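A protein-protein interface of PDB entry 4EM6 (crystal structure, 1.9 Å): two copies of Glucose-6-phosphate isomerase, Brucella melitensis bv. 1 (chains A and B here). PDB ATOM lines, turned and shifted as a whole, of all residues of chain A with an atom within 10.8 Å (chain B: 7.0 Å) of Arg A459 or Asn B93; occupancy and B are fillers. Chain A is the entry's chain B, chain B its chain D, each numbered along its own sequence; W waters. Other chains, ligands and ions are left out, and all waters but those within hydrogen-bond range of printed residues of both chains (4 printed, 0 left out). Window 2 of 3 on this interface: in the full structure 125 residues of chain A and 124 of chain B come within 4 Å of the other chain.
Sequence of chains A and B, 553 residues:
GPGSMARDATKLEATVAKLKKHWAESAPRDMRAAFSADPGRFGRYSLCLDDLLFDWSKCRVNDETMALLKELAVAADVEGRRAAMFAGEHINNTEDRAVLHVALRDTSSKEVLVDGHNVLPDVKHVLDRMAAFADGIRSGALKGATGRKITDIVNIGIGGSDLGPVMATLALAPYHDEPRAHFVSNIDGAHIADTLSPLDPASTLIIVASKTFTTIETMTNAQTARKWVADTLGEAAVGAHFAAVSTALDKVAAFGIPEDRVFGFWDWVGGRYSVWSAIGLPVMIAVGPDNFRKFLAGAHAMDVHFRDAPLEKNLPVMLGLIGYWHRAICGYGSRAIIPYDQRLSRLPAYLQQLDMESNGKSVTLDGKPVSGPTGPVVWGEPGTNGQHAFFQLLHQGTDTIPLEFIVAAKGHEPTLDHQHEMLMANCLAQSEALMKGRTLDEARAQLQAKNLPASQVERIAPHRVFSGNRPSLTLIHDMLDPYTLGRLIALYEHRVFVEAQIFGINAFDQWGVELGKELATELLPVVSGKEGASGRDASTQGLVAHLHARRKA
Asn B93 touches Arg A459.
Ile A460 touches Thr B94 (CD1 to O, 3.3 Å).
Pro A462 touches Gly B367.
Thr B94 touches His A463 (CG2 to CE1, 3.4 Å).
His A463 touches Thr B364 (CE1 to O, 3.2 Å).
His A463 touches Leu B365 (CE1 to O, 3.6 Å).
His A463 touches Gly B367.
Printed residues of chain A that touch a printed residue of chain B: Arg A459, Ile A460, Pro A462 and His A463.
Hydrophobic or aromatic side chains of chain A within 4 Å of the printed part of chain B: Ile A460, Pro A462 and His A463.
Of the 17 printed residues of chain B, 5 touch a printed residue of chain A.
Along chain B the printed residues that touch a printed residue of chain A span positions 93 to 367.
Among the printed residues, 7 pairs touch across the chains.
The backbone carbonyl oxygen (O) of Leu B365 sits at hydrogen-bond distance from the side-chain amide nitrogen (ND2) of Asn B93 (3.0 Å).
N of Asp B366 sits close to OG1 of Thr B364 (3.5 Å).
OG1 of Thr B94 is in hydrogen-bond range of OD2 of Asp B509 (2.6 Å).
The side-chain hydroxyl of Thr B94 is in hydrogen-bond range of the side-chain amide nitrogen of Asn B506 (3.3 Å).
No position is printed for both chains.
Of chain B, only Asn B93 comes within 4 Å of Arg A459.
Of the printed residues of chain A, Asn B93 touches Arg A459.
Asn B92 touches none of the printed residues of chain A.
Thr B94 touches just these residues of chain A: Ile A460 and His A463.
Leu B365 touches just one residue of chain A: His A463 (3.6 Å).
Gly B367 touches just these residues of chain A: Pro A462 (3.5 Å) and His A463 (3.6 Å).
Printed residues of chain B within 4 Å of Pro A462: Gly B367.
Printed residues of chain B within 4 Å of His A463: Thr B94 (3.4 Å), Thr B364 (3.2 Å), Leu B365 (3.6 Å) and Gly B367 (3.6 Å).
Of the printed residues of chain A, Thr B364 touches His A463 (3.2 Å).
Printed residues of chain B within 4 Å of Ile A460: Thr B94.
Ala A443 touches none of the printed residues of chain B.
Leu A440 touches none of the printed residues of chain B.
The nearest residue of chain A that does not touch Asn B93 is Ile A460 (4.9 Å).
The nearest printed residue of chain B that does not touch His A463 is Asp B509 (4.4 Å).
Water W4 lies within hydrogen-bond range of NE2 of His A463 (2.7 Å), O of Leu B365 (3.0 Å) and O of Arg A459 (3.2 Å).
Water W1 lies within hydrogen-bond range of NH2 of Arg A459 (2.8 Å), O of Thr B94 (3.2 Å) and O of Asn B93 (3.4 Å).
Water W2 lies within hydrogen-bond range of a ring nitrogen (ND1) of His A463 (2.8 Å) and the side-chain carboxylate of Asp B509 (2.8 Å).
Water W3 bridges NH2 of Arg A459 and ND2 of Asn B93.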
ATOM      1  N   LEU A 440       4.020  -8.756  21.555  1.00  0.00           N
ATOM      2  CA  LEU A 440       4.904  -8.699  22.715  1.00  0.00           C
ATOM      3  C   LEU A 440       5.006 -10.077  23.367  1.00  0.00           C
ATOM      4  O   LEU A 440       6.094 -10.523  23.739  1.00  0.00           O
ATOM      5  CB  LEU A 440       4.401  -7.671  23.729  1.00  0.00           C
ATOM      6  CG  LEU A 440       5.191  -7.504  25.038  1.00  0.00           C
ATOM      7  CD1 LEU A 440       6.635  -7.093  24.745  1.00  0.00           C
ATOM      8  CD2 LEU A 440       4.493  -6.490  25.971  1.00  0.00           C
ATOM      9  N   ALA A 443       7.238 -12.223  21.214  1.00  0.00           N
ATOM     10  CA  ALA A 443       8.629 -11.744  21.353  1.00  0.00           C
ATOM     11  C   ALA A 443       9.204 -12.199  22.673  1.00  0.00           C
ATOM     12  O   ALA A 443      10.349 -12.645  22.766  1.00  0.00           O
ATOM     13  CB  ALA A 443       8.693 -10.207  21.261  1.00  0.00           C
ATOM     14  N   ARG A 444       8.404 -12.066  23.721  1.00  0.00           N
ATOM     15  CA  ARG A 444       8.815 -12.481  25.034  1.00  0.00           C
ATOM     16  C   ARG A 444       9.147 -13.975  25.066  1.00  0.00           C
ATOM     17  O   ARG A 444      10.181 -14.379  25.628  1.00  0.00           O
ATOM     18  CB  ARG A 444       7.678 -12.160  26.010  1.00  0.00           C
ATOM     19  CG  ARG A 444       7.999 -12.358  27.458  1.00  0.00           C
ATOM     20  CD  ARG A 444       6.728 -12.062  28.304  1.00  0.00           C
ATOM     21  NE  ARG A 444       6.424 -10.630  28.438  1.00  0.00           N
ATOM     22  CZ  ARG A 444       5.230 -10.056  28.266  1.00  0.00           C
ATOM     23  NH1 ARG A 444       4.170 -10.764  27.881  1.00  0.00           N
ATOM     24  NH2 ARG A 444       5.100  -8.750  28.476  1.00  0.00           N
ATOM     25  N   LEU A 447      12.540 -14.968  23.581  1.00  0.00           N
ATOM     26  CA  LEU A 447      13.624 -14.624  24.521  1.00  0.00           C
ATOM     27  C   LEU A 447      13.692 -15.571  25.729  1.00  0.00           C
ATOM     28  O   LEU A 447      14.783 -15.960  26.166  1.00  0.00           O
ATOM     29  CB  LEU A 447      13.475 -13.163  24.979  1.00  0.00           C
ATOM     30  CG  LEU A 447      13.691 -12.107  23.884  1.00  0.00           C
ATOM     31  CD1 LEU A 447      13.507 -10.707  24.442  1.00  0.00           C
ATOM     32  CD2 LEU A 447      15.049 -12.248  23.172  1.00  0.00           C
ATOM     33  N   GLN A 448      12.527 -15.935  26.271  1.00  0.00           N
ATOM     34  CA  GLN A 448      12.446 -16.897  27.358  1.00  0.00           C
ATOM     35  C   GLN A 448      12.992 -18.264  26.961  1.00  0.00           C
ATOM     36  O   GLN A 448      13.565 -18.961  27.792  1.00  0.00           O
ATOM     37  CB  GLN A 448      11.009 -17.085  27.808  1.00  0.00           C
ATOM     38  CG  GLN A 448      10.490 -15.929  28.544  1.00  0.00           C
ATOM     39  CD  GLN A 448       9.008 -16.030  28.854  1.00  0.00           C
ATOM     40  OE1 GLN A 448       8.239 -16.689  28.126  1.00  0.00           O
ATOM     41  NE2 GLN A 448       8.587 -15.342  29.921  1.00  0.00           N
ATOM     42  N   LEU A 452      17.176 -16.238  28.927  1.00  0.00           N
ATOM     43  CA  LEU A 452      17.774 -14.993  29.392  1.00  0.00           C
ATOM     44  C   LEU A 452      17.147 -14.665  30.749  1.00  0.00           C
ATOM     45  O   LEU A 452      16.012 -15.059  31.005  1.00  0.00           O
ATOM     46  CB  LEU A 452      17.524 -13.863  28.371  1.00  0.00           C
ATOM     47  CG  LEU A 452      18.041 -14.078  26.941  1.00  0.00           C
ATOM     48  CD1 LEU A 452      17.638 -12.913  26.022  1.00  0.00           C
ATOM     49  CD2 LEU A 452      19.553 -14.278  26.890  1.00  0.00           C
ATOM     50  N   PRO A 453      17.878 -13.941  31.621  1.00  0.00           N
ATOM     51  CA  PRO A 453      17.294 -13.479  32.882  1.00  0.00           C
ATOM     52  C   PRO A 453      15.991 -12.744  32.632  1.00  0.00           C
ATOM     53  O   PRO A 453      15.866 -12.050  31.616  1.00  0.00           O
ATOM     54  CB  PRO A 453      18.345 -12.510  33.432  1.00  0.00           C
ATOM     55  CG  PRO A 453      19.626 -12.933  32.797  1.00  0.00           C
ATOM     56  CD  PRO A 453      19.265 -13.468  31.444  1.00  0.00           C
ATOM     57  N   ALA A 454      15.029 -12.918  33.531  1.00  0.00           N
ATOM     58  CA  ALA A 454      13.714 -12.305  33.383  1.00  0.00           C
ATOM     59  C   ALA A 454      13.782 -10.797  33.101  1.00  0.00           C
ATOM     60  O   ALA A 454      12.997 -10.285  32.308  1.00  0.00           O
ATOM     61  CB  ALA A 454      12.847 -12.575  34.642  1.00  0.00           C
ATOM     62  N   SER A 455      14.696 -10.071  33.748  1.00  0.00           N
ATOM     63  CA  SER A 455      14.737  -8.607  33.540  1.00  0.00           C
ATOM     64  C   SER A 455      15.175  -8.266  32.110  1.00  0.00           C
ATOM     65  O   SER A 455      14.703  -7.300  31.518  1.00  0.00           O
ATOM     66  CB  SER A 455      15.629  -7.909  34.578  1.00  0.00           C
ATOM     67  OG  SER A 455      16.973  -8.313  34.447  1.00  0.00           O
ATOM     68  N   GLN A 456      16.063  -9.084  31.562  1.00  0.00           N
ATOM     69  CA  GLN A 456      16.543  -8.898  30.205  1.00  0.00           C
ATOM     70  C   GLN A 456      15.452  -9.231  29.184  1.00  0.00           C
ATOM     71  O   GLN A 456      15.251  -8.487  28.233  1.00  0.00           O
ATOM     72  CB  GLN A 456      17.787  -9.737  29.954  1.00  0.00           C
ATOM     73  CG  GLN A 456      18.348  -9.577  28.539  1.00  0.00           C
ATOM     74  CD  GLN A 456      19.702 -10.251  28.350  1.00  0.00           C
ATOM     75  OE1 GLN A 456      20.221 -10.885  29.267  1.00  0.00           O
ATOM     76  NE2 GLN A 456      20.271 -10.127  27.151  1.00  0.00           N
ATOM     77  N   VAL A 457      14.751 -10.349  29.373  1.00  0.00           N
ATOM     78  CA  VAL A 457      13.570 -10.646  28.547  1.00  0.00           C
ATOM     79  C   VAL A 457      12.626  -9.443  28.511  1.00  0.00           C
ATOM     80  O   VAL A 457      12.197  -9.028  27.438  1.00  0.00           O
ATOM     81  CB  VAL A 457      12.778 -11.838  29.053  1.00  0.00           C
ATOM     82  CG1 VAL A 457      11.460 -11.969  28.288  1.00  0.00           C
ATOM     83  CG2 VAL A 457      13.606 -13.116  28.936  1.00  0.00           C
ATOM     84  N   GLU A 458      12.315  -8.889  29.684  1.00  0.00           N
ATOM     85  CA  GLU A 458      11.312  -7.829  29.780  1.00  0.00           C
ATOM     86  C   GLU A 458      11.826  -6.564  29.107  1.00  0.00           C
ATOM     87  O   GLU A 458      11.072  -5.854  28.437  1.00  0.00           O
ATOM     88  CB  GLU A 458      10.892  -7.589  31.249  1.00  0.00           C
ATOM     89  CG  GLU A 458      10.092  -6.308  31.436  1.00  0.00           C
ATOM     90  CD  GLU A 458       9.336  -6.215  32.773  1.00  0.00           C
ATOM     91  OE1 GLU A 458       9.483  -7.108  33.651  1.00  0.00           O
ATOM     92  OE2 GLU A 458       8.591  -5.212  32.931  1.00  0.00           O
ATOM     93  N   ARG A 459      13.120  -6.309  29.258  1.00  0.00           N
ATOM     94  CA  ARG A 459      13.764  -5.149  28.654  1.00  0.00           C
ATOM     95  C   ARG A 459      13.825  -5.220  27.130  1.00  0.00           C
ATOM     96  O   ARG A 459      13.539  -4.243  26.464  1.00  0.00           O
ATOM     97  CB  ARG A 459      15.187  -5.019  29.205  1.00  0.00           C
ATOM     98  CG  ARG A 459      15.950  -3.801  28.719  1.00  0.00           C
ATOM     99  CD  ARG A 459      17.198  -3.499  29.600  1.00  0.00           C
ATOM    100  NE  ARG A 459      17.940  -4.708  29.922  1.00  0.00           N
ATOM    101  CZ  ARG A 459      18.778  -5.349  29.103  1.00  0.00           C
ATOM    102  NH1 ARG A 459      19.380  -6.459  29.537  1.00  0.00           N
ATOM    103  NH2 ARG A 459      19.030  -4.903  27.868  1.00  0.00           N
ATOM    104  N   ILE A 460      14.216  -6.372  26.580  1.00  0.00           N
ATOM    105  CA  ILE A 460      14.445  -6.490  25.131  1.00  0.00           C
ATOM    106  C   ILE A 460      13.161  -6.745  24.346  1.00  0.00           C
ATOM    107  O   ILE A 460      13.031  -6.281  23.224  1.00  0.00           O
ATOM    108  CB  ILE A 460      15.477  -7.617  24.794  1.00  0.00           C
ATOM    109  CG1 ILE A 460      16.817  -7.345  25.480  1.00  0.00           C
ATOM    110  CG2 ILE A 460      15.675  -7.793  23.280  1.00  0.00           C
ATOM    111  CD1 ILE A 460      17.312  -5.926  25.323  1.00  0.00           C
ATOM    112  N   ALA A 461      12.206  -7.454  24.941  1.00  0.00           N
ATOM    113  CA  ALA A 461      11.013  -7.872  24.207  1.00  0.00           C
ATOM    114  C   ALA A 461      10.309  -6.765  23.379  1.00  0.00           C
ATOM    115  O   ALA A 461       9.975  -6.992  22.216  1.00  0.00           O
ATOM    116  CB  ALA A 461      10.038  -8.550  25.146  1.00  0.00           C
ATOM    117  N   PRO A 462      10.066  -5.585  23.968  1.00  0.00           N
ATOM    118  CA  PRO A 462       9.351  -4.535  23.216  1.00  0.00           C
ATOM    119  C   PRO A 462      10.051  -4.108  21.928  1.00  0.00           C
ATOM    120  O   PRO A 462       9.395  -3.626  20.976  1.00  0.00           O
ATOM    121  CB  PRO A 462       9.335  -3.365  24.200  1.00  0.00           C
ATOM    122  CG  PRO A 462       9.520  -3.991  25.531  1.00  0.00           C
ATOM    123  CD  PRO A 462      10.442  -5.124  25.312  1.00  0.00           C
ATOM    124  N   HIS A 463      11.378  -4.265  21.893  1.00  0.00           N
ATOM    125  CA  HIS A 463      12.171  -3.898  20.708  1.00  0.00           C
ATOM    126  C   HIS A 463      12.015  -4.884  19.573  1.00  0.00           C
ATOM    127  O   HIS A 463      12.400  -4.583  18.451  1.00  0.00           O
ATOM    128  CB  HIS A 463      13.661  -3.766  21.065  1.00  0.00           C
ATOM    129  CG  HIS A 463      13.928  -2.714  22.092  1.00  0.00           C
ATOM    130  ND1 HIS A 463      14.201  -1.403  21.763  1.00  0.00           N
ATOM    131  CD2 HIS A 463      13.931  -2.774  23.443  1.00  0.00           C
ATOM    132  CE1 HIS A 463      14.362  -0.702  22.868  1.00  0.00           C
ATOM    133  NE2 HIS A 463      14.208  -1.508  23.905  1.00  0.00           N
ATOM    134  N   ARG A 464      11.485  -6.069  19.886  1.00  0.00           N
ATOM    135  CA  ARG A 464      11.294  -7.146  18.914  1.00  0.00           C
ATOM    136  C   ARG A 464       9.821  -7.308  18.497  1.00  0.00           C
ATOM    137  O   ARG A 464       9.445  -8.348  17.944  1.00  0.00           O
ATOM    138  CB  ARG A 464      11.821  -8.451  19.522  1.00  0.00           C
ATOM    139  CG  ARG A 464      13.286  -8.359  19.936  1.00  0.00           C
ATOM    140  CD  ARG A 464      13.875  -9.699  20.422  1.00  0.00           C
ATOM    141  NE  ARG A 464      13.965 -10.640  19.315  1.00  0.00           N
ATOM    142  CZ  ARG A 464      13.150 -11.674  19.110  1.00  0.00           C
ATOM    143  NH1 ARG A 464      12.154 -11.957  19.949  1.00  0.00           N
ATOM    144  NH2 ARG A 464      13.332 -12.437  18.040  1.00  0.00           N
ATOM    145  N   VAL A 465       8.996  -6.291  18.773  1.00  0.00           N
ATOM    146  CA  VAL A 465       7.584  -6.299  18.402  1.00  0.00           C
ATOM    147  C   VAL A 465       7.438  -5.709  16.994  1.00  0.00           C
ATOM    148  O   VAL A 465       8.134  -4.761  16.631  1.00  0.00           O
ATOM    149  CB  VAL A 465       6.746  -5.505  19.431  1.00  0.00           C
ATOM    150  CG1 VAL A 465       5.298  -5.270  18.928  1.00  0.00           C
ATOM    151  CG2 VAL A 465       6.752  -6.225  20.771  1.00  0.00           C
ATOM    152  N   HIS B  90      28.386   1.696  26.341  1.00  0.00           N
ATOM    153  CA  HIS B  90      27.583   0.719  25.620  1.00  0.00           C
ATOM    154  C   HIS B  90      26.254   1.362  25.180  1.00  0.00           C
ATOM    155  O   HIS B  90      25.164   0.966  25.639  1.00  0.00           O
ATOM    156  CB  HIS B  90      27.335  -0.509  26.492  1.00  0.00           C
ATOM    157  CG  HIS B  90      28.558  -1.319  26.782  1.00  0.00           C
ATOM    158  ND1 HIS B  90      28.487  -2.615  27.248  1.00  0.00           N
ATOM    159  CD2 HIS B  90      29.877  -1.024  26.688  1.00  0.00           C
ATOM    160  CE1 HIS B  90      29.710  -3.083  27.428  1.00  0.00           C
ATOM    161  NE2 HIS B  90      30.571  -2.140  27.092  1.00  0.00           N
ATOM    162  N   ILE B  91      26.341   2.353  24.290  1.00  0.00           N
ATOM    163  CA  ILE B  91      25.169   3.132  23.937  1.00  0.00           C
ATOM    164  C   ILE B  91      24.169   2.362  23.067  1.00  0.00           C
ATOM    165  O   ILE B  91      23.026   2.779  22.954  1.00  0.00           O
ATOM    166  CB  ILE B  91      25.505   4.508  23.281  1.00  0.00           C
ATOM    167  CG1 ILE B  91      26.086   4.338  21.885  1.00  0.00           C
ATOM    168  CG2 ILE B  91      26.437   5.369  24.220  1.00  0.00           C
ATOM    169  CD1 ILE B  91      26.187   5.639  21.132  1.00  0.00           C
ATOM    170  N   ASN B  92      24.620   1.277  22.439  1.00  0.00           N
ATOM    171  CA  ASN B  92      23.731   0.303  21.820  1.00  0.00           C
ATOM    172  C   ASN B  92      23.227  -0.570  22.973  1.00  0.00           C
ATOM    173  O   ASN B  92      23.792  -1.618  23.295  1.00  0.00           O
ATOM    174  CB  ASN B  92      24.464  -0.499  20.738  1.00  0.00           C
ATOM    175  CG  ASN B  92      23.602  -1.544  20.093  1.00  0.00           C
ATOM    176  OD1 ASN B  92      22.438  -1.710  20.454  1.00  0.00           O
ATOM    177  ND2 ASN B  92      24.188  -2.316  19.157  1.00  0.00           N
ATOM    178  N   ASN B  93      22.167  -0.094  23.610  1.00  0.00           N
ATOM    179  CA  ASN B  93      21.735  -0.650  24.873  1.00  0.00           C
ATOM    180  C   ASN B  93      21.009  -1.977  24.755  1.00  0.00           C
ATOM    181  O   ASN B  93      21.093  -2.815  25.670  1.00  0.00           O
ATOM    182  CB  ASN B  93      20.890   0.364  25.657  1.00  0.00           C
ATOM    183  CG  ASN B  93      19.599   0.735  24.947  1.00  0.00           C
ATOM    184  OD1 ASN B  93      19.603   1.098  23.777  1.00  0.00           O
ATOM    185  ND2 ASN B  93      18.492   0.626  25.654  1.00  0.00           N
ATOM    186  N   THR B  94      20.300  -2.182  23.643  1.00  0.00           N
ATOM    187  CA  THR B  94      19.491  -3.378  23.466  1.00  0.00           C
ATOM    188  C   THR B  94      20.367  -4.585  23.162  1.00  0.00           C
ATOM    189  O   THR B  94      20.017  -5.711  23.523  1.00  0.00           O
ATOM    190  CB  THR B  94      18.421  -3.186  22.378  1.00  0.00           C
ATOM    191  OG1 THR B  94      19.048  -2.977  21.107  1.00  0.00           O
ATOM    192  CG2 THR B  94      17.539  -1.981  22.732  1.00  0.00           C
ATOM    193  N   GLU B  95      21.517  -4.343  22.538  1.00  0.00           N
ATOM    194  CA  GLU B  95      22.515  -5.385  22.304  1.00  0.00           C
ATOM    195  C   GLU B  95      23.676  -5.329  23.307  1.00  0.00           C
ATOM    196  O   GLU B  95      24.510  -6.228  23.335  1.00  0.00           O
ATOM    197  CB  GLU B  95      23.037  -5.275  20.873  1.00  0.00           C
ATOM    198  CG  GLU B  95      21.943  -5.569  19.871  1.00  0.00           C
ATOM    199  CD  GLU B  95      22.393  -5.532  18.428  1.00  0.00           C
ATOM    200  OE1 GLU B  95      23.055  -4.543  18.050  1.00  0.00           O
ATOM    201  OE2 GLU B  95      22.058  -6.483  17.673  1.00  0.00           O
ATOM    202  N   ASP B  96      23.695  -4.290  24.144  1.00  0.00           N
ATOM    203  CA  ASP B  96      24.752  -4.067  25.133  1.00  0.00           C
ATOM    204  C   ASP B  96      26.112  -4.067  24.483  1.00  0.00           C
ATOM    205  O   ASP B  96      26.960  -4.915  24.756  1.00  0.00           O
ATOM    206  CB  ASP B  96      24.711  -5.095  26.257  1.00  0.00           C
ATOM    207  CG  ASP B  96      25.643  -4.738  27.405  1.00  0.00           C
ATOM    208  OD1 ASP B  96      26.016  -3.541  27.571  1.00  0.00           O
ATOM    209  OD2 ASP B  96      25.998  -5.666  28.138  1.00  0.00           O
ATOM    210  N   ARG B  97      26.285  -3.120  23.574  1.00  0.00           N
ATOM    211  CA  ARG B  97      27.527  -2.966  22.844  1.00  0.00           C
ATOM    212  C   ARG B  97      27.930  -1.509  22.774  1.00  0.00           C
ATOM    213  O   ARG B  97      27.083  -0.603  22.815  1.00  0.00           O
ATOM    214  CB  ARG B  97      27.370  -3.455  21.419  1.00  0.00           C
ATOM    215  CG  ARG B  97      27.248  -4.928  21.277  1.00  0.00           C
ATOM    216  CD  ARG B  97      26.996  -5.309  19.822  1.00  0.00           C
ATOM    217  NE  ARG B  97      26.480  -6.668  19.744  1.00  0.00           N
ATOM    218  CZ  ARG B  97      26.044  -7.257  18.633  1.00  0.00           C
ATOM    219  NH1 ARG B  97      26.067  -6.637  17.464  1.00  0.00           N
ATOM    220  NH2 ARG B  97      25.578  -8.492  18.695  1.00  0.00           N
ATOM    221  N   VAL B  99      29.729   1.479  20.403  1.00  0.00           N
ATOM    222  CA  VAL B  99      29.472   1.940  19.057  1.00  0.00           C
ATOM    223  C   VAL B  99      30.679   2.776  18.667  1.00  0.00           C
ATOM    224  O   VAL B  99      30.787   3.961  19.024  1.00  0.00           O
ATOM    225  CB  VAL B  99      28.198   2.781  19.004  1.00  0.00           C
ATOM    226  CG1 VAL B  99      28.031   3.419  17.614  1.00  0.00           C
ATOM    227  CG2 VAL B  99      26.981   1.915  19.385  1.00  0.00           C
ATOM    228  N   THR B 364      11.545   3.722  21.788  1.00  0.00           N
ATOM    229  CA  THR B 364      12.637   4.504  22.337  1.00  0.00           C
ATOM    230  C   THR B 364      13.669   3.573  22.982  1.00  0.00           C
ATOM    231  O   THR B 364      13.443   2.356  23.091  1.00  0.00           O
ATOM    232  CB  THR B 364      12.113   5.474  23.431  1.00  0.00           C
ATOM    233  OG1 THR B 364      11.542   4.706  24.490  1.00  0.00           O
ATOM    234  CG2 THR B 364      11.060   6.420  22.882  1.00  0.00           C
ATOM    235  N   LEU B 365      14.781   4.138  23.431  1.00  0.00           N
ATOM    236  CA  LEU B 365      15.816   3.358  24.128  1.00  0.00           C
ATOM    237  C   LEU B 365      15.215   2.545  25.277  1.00  0.00           C
ATOM    238  O   LEU B 365      15.603   1.389  25.494  1.00  0.00           O
ATOM    239  CB  LEU B 365      16.916   4.272  24.680  1.00  0.00           C
ATOM    240  CG  LEU B 365      17.775   5.078  23.700  1.00  0.00           C
ATOM    241  CD1 LEU B 365      18.699   6.018  24.468  1.00  0.00           C
ATOM    242  CD2 LEU B 365      18.597   4.181  22.793  1.00  0.00           C
ATOM    243  N   ASP B 366      14.258   3.131  25.994  1.00  0.00           N
ATOM    244  CA  ASP B 366      13.665   2.484  27.168  1.00  0.00           C
ATOM    245  C   ASP B 366      12.500   1.547  26.808  1.00  0.00           C
ATOM    246  O   ASP B 366      11.821   1.056  27.691  1.00  0.00           O
ATOM    247  CB  ASP B 366      13.256   3.528  28.246  1.00  0.00           C
ATOM    248  CG  ASP B 366      12.001   4.348  27.892  1.00  0.00           C
ATOM    249  OD1 ASP B 366      11.649   4.481  26.694  1.00  0.00           O
ATOM    250  OD2 ASP B 366      11.344   4.888  28.842  1.00  0.00           O
ATOM    251  N   GLY B 367      12.291   1.300  25.516  1.00  0.00           N
ATOM    252  CA  GLY B 367      11.305   0.332  25.079  1.00  0.00           C
ATOM    253  C   GLY B 367       9.880   0.856  25.024  1.00  0.00           C
ATOM    254  O   GLY B 367       8.958   0.063  24.870  1.00  0.00           O
ATOM    255  N   ILE B 505      15.770   7.125  20.016  1.00  0.00           N
ATOM    256  CA  ILE B 505      15.830   5.717  19.598  1.00  0.00           C
ATOM    257  C   ILE B 505      17.266   5.196  19.595  1.00  0.00           C
ATOM    258  O   ILE B 505      18.226   5.957  19.742  1.00  0.00           O
ATOM    259  CB  ILE B 505      15.215   5.499  18.179  1.00  0.00           C
ATOM    260  CG1 ILE B 505      15.999   6.267  17.103  1.00  0.00           C
ATOM    261  CG2 ILE B 505      13.743   5.865  18.184  1.00  0.00           C
ATOM    262  CD1 ILE B 505      15.385   6.196  15.688  1.00  0.00           C
ATOM    263  N   ASN B 506      17.413   3.893  19.435  1.00  0.00           N
ATOM    264  CA  ASN B 506      18.729   3.292  19.282  1.00  0.00           C
ATOM    265  C   ASN B 506      19.059   3.226  17.802  1.00  0.00           C
ATOM    266  O   ASN B 506      18.504   2.412  17.084  1.00  0.00           O
ATOM    267  CB  ASN B 506      18.741   1.886  19.901  1.00  0.00           C
ATOM    268  CG  ASN B 506      20.146   1.260  19.941  1.00  0.00           C
ATOM    269  OD1 ASN B 506      21.118   1.866  19.504  1.00  0.00           O
ATOM    270  ND2 ASN B 506      20.230   0.025  20.449  1.00  0.00           N
ATOM    271  N   PHE B 508      21.537   1.943  16.498  1.00  0.00           N
ATOM    272  CA  PHE B 508      22.625   0.964  16.277  1.00  0.00           C
ATOM    273  C   PHE B 508      22.202  -0.513  16.349  1.00  0.00           C
ATOM    274  O   PHE B 508      23.017  -1.404  16.086  1.00  0.00           O
ATOM    275  CB  PHE B 508      23.822   1.299  17.205  1.00  0.00           C
ATOM    276  CG  PHE B 508      24.321   2.701  16.992  1.00  0.00           C
ATOM    277  CD1 PHE B 508      24.963   3.030  15.799  1.00  0.00           C
ATOM    278  CD2 PHE B 508      24.037   3.705  17.897  1.00  0.00           C
ATOM    279  CE1 PHE B 508      25.347   4.342  15.525  1.00  0.00           C
ATOM    280  CE2 PHE B 508      24.413   5.017  17.645  1.00  0.00           C
ATOM    281  CZ  PHE B 508      25.084   5.329  16.451  1.00  0.00           C
ATOM    282  N   ASP B 509      20.928  -0.760  16.647  1.00  0.00           N
ATOM    283  CA  ASP B 509      20.368  -2.120  16.564  1.00  0.00           C
ATOM    284  C   ASP B 509      19.546  -2.274  15.279  1.00  0.00           C
ATOM    285  O   ASP B 509      19.414  -1.325  14.506  1.00  0.00           O
ATOM    286  CB  ASP B 509      19.575  -2.480  17.841  1.00  0.00           C
ATOM    287  CG  ASP B 509      18.357  -1.615  18.068  1.00  0.00           C
ATOM    288  OD1 ASP B 509      17.901  -0.909  17.127  1.00  0.00           O
ATOM    289  OD2 ASP B 509      17.824  -1.701  19.203  1.00  0.00           O
HETATM  290  O   HOH W   1      21.121  -6.072  26.474  1.00  0.00           O
HETATM  291  O   HOH W   2      15.216  -0.558  19.309  1.00  0.00           O
HETATM  292  O   HOH W   3      17.641  -2.254  26.762  1.00  0.00           O
HETATM  293  O   HOH W   4      14.568  -1.223  26.595  1.00  0.00           O
